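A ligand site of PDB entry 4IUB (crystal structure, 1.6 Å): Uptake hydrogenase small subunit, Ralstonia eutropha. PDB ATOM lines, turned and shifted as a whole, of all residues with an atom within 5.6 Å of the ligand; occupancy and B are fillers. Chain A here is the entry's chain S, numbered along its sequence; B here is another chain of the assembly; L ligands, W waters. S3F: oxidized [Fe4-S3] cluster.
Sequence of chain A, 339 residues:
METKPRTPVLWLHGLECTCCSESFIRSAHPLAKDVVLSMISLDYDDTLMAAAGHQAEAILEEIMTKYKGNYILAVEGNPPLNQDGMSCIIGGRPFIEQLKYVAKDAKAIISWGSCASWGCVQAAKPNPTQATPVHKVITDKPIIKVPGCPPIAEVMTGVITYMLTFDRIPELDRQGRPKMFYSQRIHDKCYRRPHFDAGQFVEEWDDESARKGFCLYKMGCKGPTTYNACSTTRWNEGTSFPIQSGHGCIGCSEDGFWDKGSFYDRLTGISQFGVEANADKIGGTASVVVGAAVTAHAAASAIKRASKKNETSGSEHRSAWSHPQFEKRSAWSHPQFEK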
ATOM      1  N   GLU A  16      19.643   8.148 -18.253  1.00  0.00           N
ATOM      2  CA  GLU A  16      18.824   8.828 -19.255  1.00  0.00           C
ATOM      3  C   GLU A  16      17.390   8.354 -19.181  1.00  0.00           C
ATOM      4  O   GLU A  16      17.092   7.353 -18.526  1.00  0.00           O
ATOM      5  CB  GLU A  16      19.339   8.413 -20.620  1.00  0.00           C
ATOM      6  CG  GLU A  16      19.390   6.899 -20.683  1.00  0.00           C
ATOM      7  CD  GLU A  16      19.330   6.345 -22.069  1.00  0.00           C
ATOM      8  OE1 GLU A  16      19.000   7.098 -23.006  1.00  0.00           O
ATOM      9  OE2 GLU A  16      19.588   5.129 -22.195  1.00  0.00           O
ATOM     10  N   CYS A  17      16.520   9.023 -19.936  1.00  0.00           N
ATOM     11  CA  CYS A  17      15.155   8.551 -20.125  1.00  0.00           C
ATOM     12  C   CYS A  17      14.907   8.189 -21.602  1.00  0.00           C
ATOM     13  O   CYS A  17      13.849   7.644 -21.931  1.00  0.00           O
ATOM     14  CB  CYS A  17      14.134   9.591 -19.653  1.00  0.00           C
ATOM     15  SG  CYS A  17      13.694  10.815 -20.899  1.00  0.00           S
ATOM     16  N   THR A  18      15.893   8.488 -22.462  1.00  0.00           N
ATOM     17  CA  THR A  18      15.860   8.188 -23.906  1.00  0.00           C
ATOM     18  C   THR A  18      14.991   9.149 -24.738  1.00  0.00           C
ATOM     19  O   THR A  18      14.740   8.919 -25.931  1.00  0.00           O
ATOM     20  CB  THR A  18      15.527   6.691 -24.164  1.00  0.00           C
ATOM     21  OG1 THR A  18      16.299   5.886 -23.273  1.00  0.00           O
ATOM     22  CG2 THR A  18      15.873   6.286 -25.590  1.00  0.00           C
ATOM     23  N   CYS A  19      14.560  10.248 -24.130  1.00  0.00           N
ATOM     24  CA  CYS A  19      13.795  11.273 -24.872  1.00  0.00           C
ATOM     25  C   CYS A  19      14.577  11.885 -26.042  1.00  0.00           C
ATOM     26  O   CYS A  19      13.990  12.222 -27.059  1.00  0.00           O
ATOM     27  CB  CYS A  19      13.263  12.382 -23.954  1.00  0.00           C
ATOM     28  SG  CYS A  19      14.512  13.412 -23.133  1.00  0.00           S
ATOM     29  N   CYS A  20      15.888  12.042 -25.885  1.00  0.00           N
ATOM     30  CA  CYS A  20      16.676  12.646 -26.968  1.00  0.00           C
ATOM     31  C   CYS A  20      16.719  11.732 -28.189  1.00  0.00           C
ATOM     32  O   CYS A  20      16.590  12.197 -29.340  1.00  0.00           O
ATOM     33  CB  CYS A  20      18.093  12.976 -26.491  1.00  0.00           C
ATOM     34  SG  CYS A  20      18.096  13.993 -24.986  1.00  0.00           S
ATOM     35  N   SER A  21      16.888  10.436 -27.964  1.00  0.00           N
ATOM     36  CA  SER A  21      16.871   9.483 -29.094  1.00  0.00           C
ATOM     37  C   SER A  21      15.524   9.519 -29.815  1.00  0.00           C
ATOM     38  O   SER A  21      15.458   9.449 -31.056  1.00  0.00           O
ATOM     39  CB  SER A  21      17.153   8.062 -28.611  1.00  0.00           C
ATOM     40  OG  SER A  21      18.549   7.852 -28.415  1.00  0.00           O
ATOM     41  N   GLU A  76      24.065  10.637 -24.875  1.00  0.00           N
ATOM     42  CA  GLU A  76      22.763  10.906 -24.313  1.00  0.00           C
ATOM     43  C   GLU A  76      22.819  10.427 -22.861  1.00  0.00           C
ATOM     44  O   GLU A  76      23.414   9.382 -22.575  1.00  0.00           O
ATOM     45  CB  GLU A  76      21.700  10.131 -25.093  1.00  0.00           C
ATOM     46  CG  GLU A  76      20.274  10.381 -24.661  1.00  0.00           C
ATOM     47  CD  GLU A  76      19.305   9.703 -25.599  1.00  0.00           C
ATOM     48  OE1 GLU A  76      19.740   9.215 -26.665  1.00  0.00           O
ATOM     49  OE2 GLU A  76      18.114   9.677 -25.268  1.00  0.00           O
ATOM     50  N   GLY A  77      22.240  11.186 -21.948  1.00  0.00           N
ATOM     51  CA  GLY A  77      22.331  10.832 -20.533  1.00  0.00           C
ATOM     52  C   GLY A  77      23.674  11.232 -19.936  1.00  0.00           C
ATOM     53  O   GLY A  77      24.450  11.958 -20.553  1.00  0.00           O
ATOM     54  N   TRP A 112      24.024  15.433 -26.036  1.00  0.00           N
ATOM     55  CA  TRP A 112      22.602  15.531 -26.377  1.00  0.00           C
ATOM     56  C   TRP A 112      21.788  15.808 -25.163  1.00  0.00           C
ATOM     57  O   TRP A 112      21.898  15.081 -24.176  1.00  0.00           O
ATOM     58  CB  TRP A 112      22.073  14.213 -26.908  1.00  0.00           C
ATOM     59  CG  TRP A 112      22.428  13.806 -28.323  1.00  0.00           C
ATOM     60  CD1 TRP A 112      22.763  12.515 -28.750  1.00  0.00           C
ATOM     61  CD2 TRP A 112      22.404  14.626 -29.545  1.00  0.00           C
ATOM     62  NE1 TRP A 112      22.965  12.496 -30.115  1.00  0.00           N
ATOM     63  CE2 TRP A 112      22.774  13.721 -30.649  1.00  0.00           C
ATOM     64  CE3 TRP A 112      22.152  15.969 -29.823  1.00  0.00           C
ATOM     65  CZ2 TRP A 112      22.870  14.166 -31.956  1.00  0.00           C
ATOM     66  CZ3 TRP A 112      22.248  16.404 -31.150  1.00  0.00           C
ATOM     67  CH2 TRP A 112      22.606  15.519 -32.194  1.00  0.00           C
ATOM     68  N   GLY A 113      20.936  16.821 -25.219  1.00  0.00           N
ATOM     69  CA  GLY A 113      19.932  17.031 -24.173  1.00  0.00           C
ATOM     70  C   GLY A 113      20.468  17.601 -22.878  1.00  0.00           C
ATOM     71  O   GLY A 113      21.668  17.721 -22.661  1.00  0.00           O
ATOM     72  N   SER A 114      19.544  17.949 -21.989  1.00  0.00           N
ATOM     73  CA  SER A 114      19.893  18.471 -20.685  1.00  0.00           C
ATOM     74  C   SER A 114      20.649  17.453 -19.803  1.00  0.00           C
ATOM     75  O   SER A 114      21.467  17.851 -18.988  1.00  0.00           O
ATOM     76  CB  SER A 114      18.642  19.021 -19.991  1.00  0.00           C
ATOM     77  OG  SER A 114      18.152  20.141 -20.746  1.00  0.00           O
ATOM     78  N   CYS A 115      20.384  16.159 -19.957  1.00  0.00           N
ATOM     79  CA  CYS A 115      21.120  15.158 -19.177  1.00  0.00           C
ATOM     80  C   CYS A 115      22.609  15.273 -19.428  1.00  0.00           C
ATOM     81  O   CYS A 115      23.406  15.447 -18.499  1.00  0.00           O
ATOM     82  CB  CYS A 115      20.681  13.729 -19.522  1.00  0.00           C
ATOM     83  SG  CYS A 115      19.116  13.195 -18.825  1.00  0.00           S
ATOM     84  N   CYS A 120      20.168  17.336 -15.820  1.00  0.00           N
ATOM     85  CA  CYS A 120      18.717  17.119 -15.897  1.00  0.00           C
ATOM     86  C   CYS A 120      18.134  16.465 -14.641  1.00  0.00           C
ATOM     87  O   CYS A 120      18.632  16.696 -13.534  1.00  0.00           O
ATOM     88  CB  CYS A 120      18.306  16.383 -17.201  1.00  0.00           C
ATOM     89  SG  CYS A 120      16.610  16.733 -17.766  1.00  0.00           S
ATOM     90  N   VAL A 121      17.076  15.662 -14.795  1.00  0.00           N
ATOM     91  CA  VAL A 121      16.233  15.312 -13.644  1.00  0.00           C
ATOM     92  C   VAL A 121      16.972  14.559 -12.540  1.00  0.00           C
ATOM     93  O   VAL A 121      16.791  14.844 -11.337  1.00  0.00           O
ATOM     94  CB  VAL A 121      14.903  14.611 -14.066  1.00  0.00           C
ATOM     95  CG1 VAL A 121      15.142  13.143 -14.420  1.00  0.00           C
ATOM     96  CG2 VAL A 121      13.854  14.768 -12.980  1.00  0.00           C
ATOM     97  N   GLN A 122      17.839  13.619 -12.932  1.00  0.00           N
ATOM     98  CA  GLN A 122      18.569  12.824 -11.957  1.00  0.00           C
ATOM     99  C   GLN A 122      19.565  13.648 -11.142  1.00  0.00           C
ATOM    100  O   GLN A 122      19.938  13.254 -10.036  1.00  0.00           O
ATOM    101  CB  GLN A 122      19.278  11.633 -12.618  1.00  0.00           C
ATOM    102  CG  GLN A 122      20.242  11.985 -13.750  1.00  0.00           C
ATOM    103  CD  GLN A 122      19.600  11.922 -15.118  1.00  0.00           C
ATOM    104  OE1 GLN A 122      18.415  12.225 -15.291  1.00  0.00           O
ATOM    105  NE2 GLN A 122      20.384  11.527 -16.120  1.00  0.00           N
ATOM    106  N   GLY A 148      18.022  20.862 -23.570  1.00  0.00           N
ATOM    107  CA  GLY A 148      16.593  20.727 -23.783  1.00  0.00           C
ATOM    108  C   GLY A 148      16.199  19.322 -23.399  1.00  0.00           C
ATOM    109  O   GLY A 148      17.019  18.392 -23.480  1.00  0.00           O
ATOM    110  N   CYS A 149      14.951  19.160 -22.995  1.00  0.00           N
ATOM    111  CA  CYS A 149      14.486  17.887 -22.446  1.00  0.00           C
ATOM    112  C   CYS A 149      13.199  17.425 -23.147  1.00  0.00           C
ATOM    113  O   CYS A 149      12.106  17.597 -22.627  1.00  0.00           O
ATOM    114  CB  CYS A 149      14.284  17.992 -20.928  1.00  0.00           C
ATOM    115  SG  CYS A 149      13.942  16.394 -20.142  1.00  0.00           S
ATOM    116  N   PRO A 150      13.339  16.839 -24.343  1.00  0.00           N
ATOM    117  CA  PRO A 150      14.570  16.706 -25.122  1.00  0.00           C
ATOM    118  C   PRO A 150      14.751  17.982 -25.962  1.00  0.00           C
ATOM    119  O   PRO A 150      13.874  18.846 -25.964  1.00  0.00           O
ATOM    120  CB  PRO A 150      14.273  15.506 -26.026  1.00  0.00           C
ATOM    121  CG  PRO A 150      12.780  15.590 -26.263  1.00  0.00           C
ATOM    122  CD  PRO A 150      12.173  16.252 -25.043  1.00  0.00           C
ATOM    123  N   PRO A 151      15.889  18.106 -26.669  1.00  0.00           N
ATOM    124  CA  PRO A 151      15.972  19.189 -27.662  1.00  0.00           C
ATOM    125  C   PRO A 151      14.975  18.953 -28.785  1.00  0.00           C
ATOM    126  O   PRO A 151      14.532  17.820 -28.997  1.00  0.00           O
ATOM    127  CB  PRO A 151      17.389  19.053 -28.225  1.00  0.00           C
ATOM    128  CG  PRO A 151      18.108  18.094 -27.332  1.00  0.00           C
ATOM    129  CD  PRO A 151      17.067  17.234 -26.690  1.00  0.00           C
ATOM    130  N   TRP A 258      15.242  22.276 -12.829  1.00  0.00           N
ATOM    131  CA  TRP A 258      14.408  21.538 -11.877  1.00  0.00           C
ATOM    132  C   TRP A 258      14.432  22.117 -10.494  1.00  0.00           C
ATOM    133  O   TRP A 258      13.517  21.898  -9.710  1.00  0.00           O
ATOM    134  CB  TRP A 258      14.875  20.086 -11.788  1.00  0.00           C
ATOM    135  CG  TRP A 258      14.808  19.342 -13.094  1.00  0.00           C
ATOM    136  CD1 TRP A 258      15.848  19.051 -13.980  1.00  0.00           C
ATOM    137  CD2 TRP A 258      13.603  18.770 -13.704  1.00  0.00           C
ATOM    138  NE1 TRP A 258      15.375  18.347 -15.068  1.00  0.00           N
ATOM    139  CE2 TRP A 258      14.039  18.141 -14.960  1.00  0.00           C
ATOM    140  CE3 TRP A 258      12.261  18.705 -13.346  1.00  0.00           C
ATOM    141  CZ2 TRP A 258      13.145  17.493 -15.807  1.00  0.00           C
ATOM    142  CZ3 TRP A 258      11.372  18.053 -14.206  1.00  0.00           C
ATOM    143  CH2 TRP A 258      11.809  17.462 -15.411  1.00  0.00           C
ATOM    144  N   ARG B  53      18.320   6.084 -11.068  1.00  0.00           N
ATOM    145  CA  ARG B  53      18.424   7.556 -10.993  1.00  0.00           C
ATOM    146  C   ARG B  53      17.869   8.113  -9.684  1.00  0.00           C
ATOM    147  O   ARG B  53      18.355   9.129  -9.200  1.00  0.00           O
ATOM    148  CB  ARG B  53      17.725   8.210 -12.203  1.00  0.00           C
ATOM    149  CG  ARG B  53      18.523   8.086 -13.509  1.00  0.00           C
ATOM    150  CD  ARG B  53      17.692   8.422 -14.750  1.00  0.00           C
ATOM    151  NE  ARG B  53      16.565   7.507 -14.872  1.00  0.00           N
ATOM    152  CZ  ARG B  53      15.381   7.790 -15.450  1.00  0.00           C
ATOM    153  NH1 ARG B  53      15.169   8.975 -16.010  1.00  0.00           N
ATOM    154  NH2 ARG B  53      14.410   6.870 -15.426  1.00  0.00           N
ATOM    155  N   ARG B  73       9.839  12.421 -16.822  1.00  0.00           N
ATOM    156  CA  ARG B  73      11.224  12.153 -17.230  1.00  0.00           C
ATOM    157  C   ARG B  73      11.782  10.842 -16.702  1.00  0.00           C
ATOM    158  O   ARG B  73      12.955  10.561 -16.851  1.00  0.00           O
ATOM    159  CB  ARG B  73      12.148  13.304 -16.835  1.00  0.00           C
ATOM    160  CG  ARG B  73      12.207  14.435 -17.855  1.00  0.00           C
ATOM    161  CD  ARG B  73      10.857  15.118 -18.064  1.00  0.00           C
ATOM    162  NE  ARG B  73      11.014  16.225 -19.003  1.00  0.00           N
ATOM    163  CZ  ARG B  73      10.095  17.145 -19.268  1.00  0.00           C
ATOM    164  NH1 ARG B  73       8.918  17.154 -18.638  1.00  0.00           N
ATOM    165  NH2 ARG B  73      10.376  18.082 -20.171  1.00  0.00           N
ATOM    166  N   GLY B  76      11.252   8.655 -21.782  1.00  0.00           N
ATOM    167  CA  GLY B  76      10.891   9.401 -22.993  1.00  0.00           C
ATOM    168  C   GLY B  76      10.332   8.504 -24.085  1.00  0.00           C
ATOM    169  O   GLY B  76       9.916   8.997 -25.138  1.00  0.00           O
ATOM    170  N   HIS B 229       7.708  14.197 -24.279  1.00  0.00           N
ATOM    171  CA  HIS B 229       7.448  14.936 -23.022  1.00  0.00           C
ATOM    172  C   HIS B 229       6.412  16.039 -23.142  1.00  0.00           C
ATOM    173  O   HIS B 229       6.681  17.185 -22.810  1.00  0.00           O
ATOM    174  CB  HIS B 229       8.758  15.434 -22.392  1.00  0.00           C
ATOM    175  CG  HIS B 229       9.655  14.316 -21.906  1.00  0.00           C
ATOM    176  ND1 HIS B 229       9.177  13.094 -21.534  1.00  0.00           N
ATOM    177  CD2 HIS B 229      11.029  14.277 -21.701  1.00  0.00           C
ATOM    178  CE1 HIS B 229      10.208  12.326 -21.116  1.00  0.00           C
ATOM    179  NE2 HIS B 229      11.342  13.050 -21.215  1.00  0.00           N
HETATM  180  S2  S3F L   1      15.600  13.301 -19.196  1.00  0.00           S
HETATM  181 FE2  S3F L   1      17.535  13.337 -20.497  1.00  0.00          FE
HETATM  182  S3  S3F L   1      17.381  15.351 -21.387  1.00  0.00           S
HETATM  183 FE3  S3F L   1      15.974  15.453 -19.663  1.00  0.00          FE
HETATM  184  S1  S3F L   1      17.513  11.646 -21.988  1.00  0.00           S
HETATM  185 FE1  S3F L   1      15.279  12.384 -21.210  1.00  0.00          FE
HETATM  186  O1  S3F L   1      13.713  13.215 -20.814  1.00  0.00           O
HETATM  187 FE4  S3F L   1      16.614  12.550 -23.978  1.00  0.00          FE
HETATM  188  O   HOH W   1      16.977  10.893 -17.108  1.00  0.00           O
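S3 of the ligand lies close to O of Gly 148. Glu 16 touches the ligand. Glu 76 of chain A touches the ligand. Arg 73 of chain B touches the ligand. Hydrophobic or aromatic side chains that line the ligand: His 229 of chain B. Within 4 Å of the ligand: Glu 16, Cys 17, Thr 18, Cys 19, Cys 20, Glu 76 of chain A, Ser 114, Cys 115, Cys 120, Gly 148, Cys 149, Arg 73 of chain B and His 229 of chain B. The nearest printed residue that does not touch the ligand is Gly 113 (4.1 Å).
Water W1 lies within hydrogen-bond range of the side-chain amide oxygen (OE1) of Gln 122, the guanidinium group (NH1) of Arg 53 of chain B, the backbone NH (N) of Cys 17 and a sulfur (S2) of the ligand.
S1 of the ligand lies close to N of Thr 18 (3.6 Å). N of Cys 20 binds FE4 of the ligand, 2.1 Å away. SG of Cys 115 binds FE2 of the ligand, at 2.3 Å. FE3 of the ligand is bound by SG of Cys 120 (2.4 Å). SG of Cys 17 binds FE1 of the ligand (2.3 Å). The side-chain sulfur (SG) of Cys 20 binds an iron atom (FE4) of the ligand (2.3 Å). An oxygen (O1) of the ligand lies close to a ring nitrogen (NE2) of His 229 of chain B (2.4 Å). A sulfur (S3) of the ligand lies close to the backbone NH (N) of Ser 114. The backbone NH (N) of Cys 17 lies close to a sulfur (S1) of the ligand (3.5 Å). The side-chain sulfur (SG) of Cys 19 is bound to an iron atom (FE1) of the ligand (2.3 Å). The side-chain sulfur (SG) of Cys 149 binds an iron atom (FE3) of the ligand (2.3 Å). The backbone NH (N) of Cys 115 lies close to a sulfur (S3) of the ligand (3.4 Å).
The side-chain sulfur (SG) of Cys 120 lies close to the indole nitrogen (NE1) of Trp 258 (3.4 Å). SG of Cys 115 lies close to NE2 of Gln 122. OE1 of Glu 76 of chain A is in hydrogen-bond range of OG of Ser 21 (2.5 Å). The backbone NH of Cys 120 is in hydrogen-bond range of the backbone carbonyl oxygen of Ser 114, at 3.5 Å. The guanidinium group (NH1) of Arg 53 of chain B sits at hydrogen-bond distance from the backbone carbonyl oxygen (O) of Arg 73 of chain B, 2.9 Å away. The side-chain sulfur of Cys 19 lies close to a ring nitrogen (NE2) of His 229 of chain B (3.7 Å). The backbone carbonyl oxygen (O) of Cys 17 sits at hydrogen-bond distance from the backbone NH (N) of Gly 76 of chain B, at 2.8 Å. OG of Ser 114 sits at hydrogen-bond distance from N of Gly 148 (2.9 Å).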
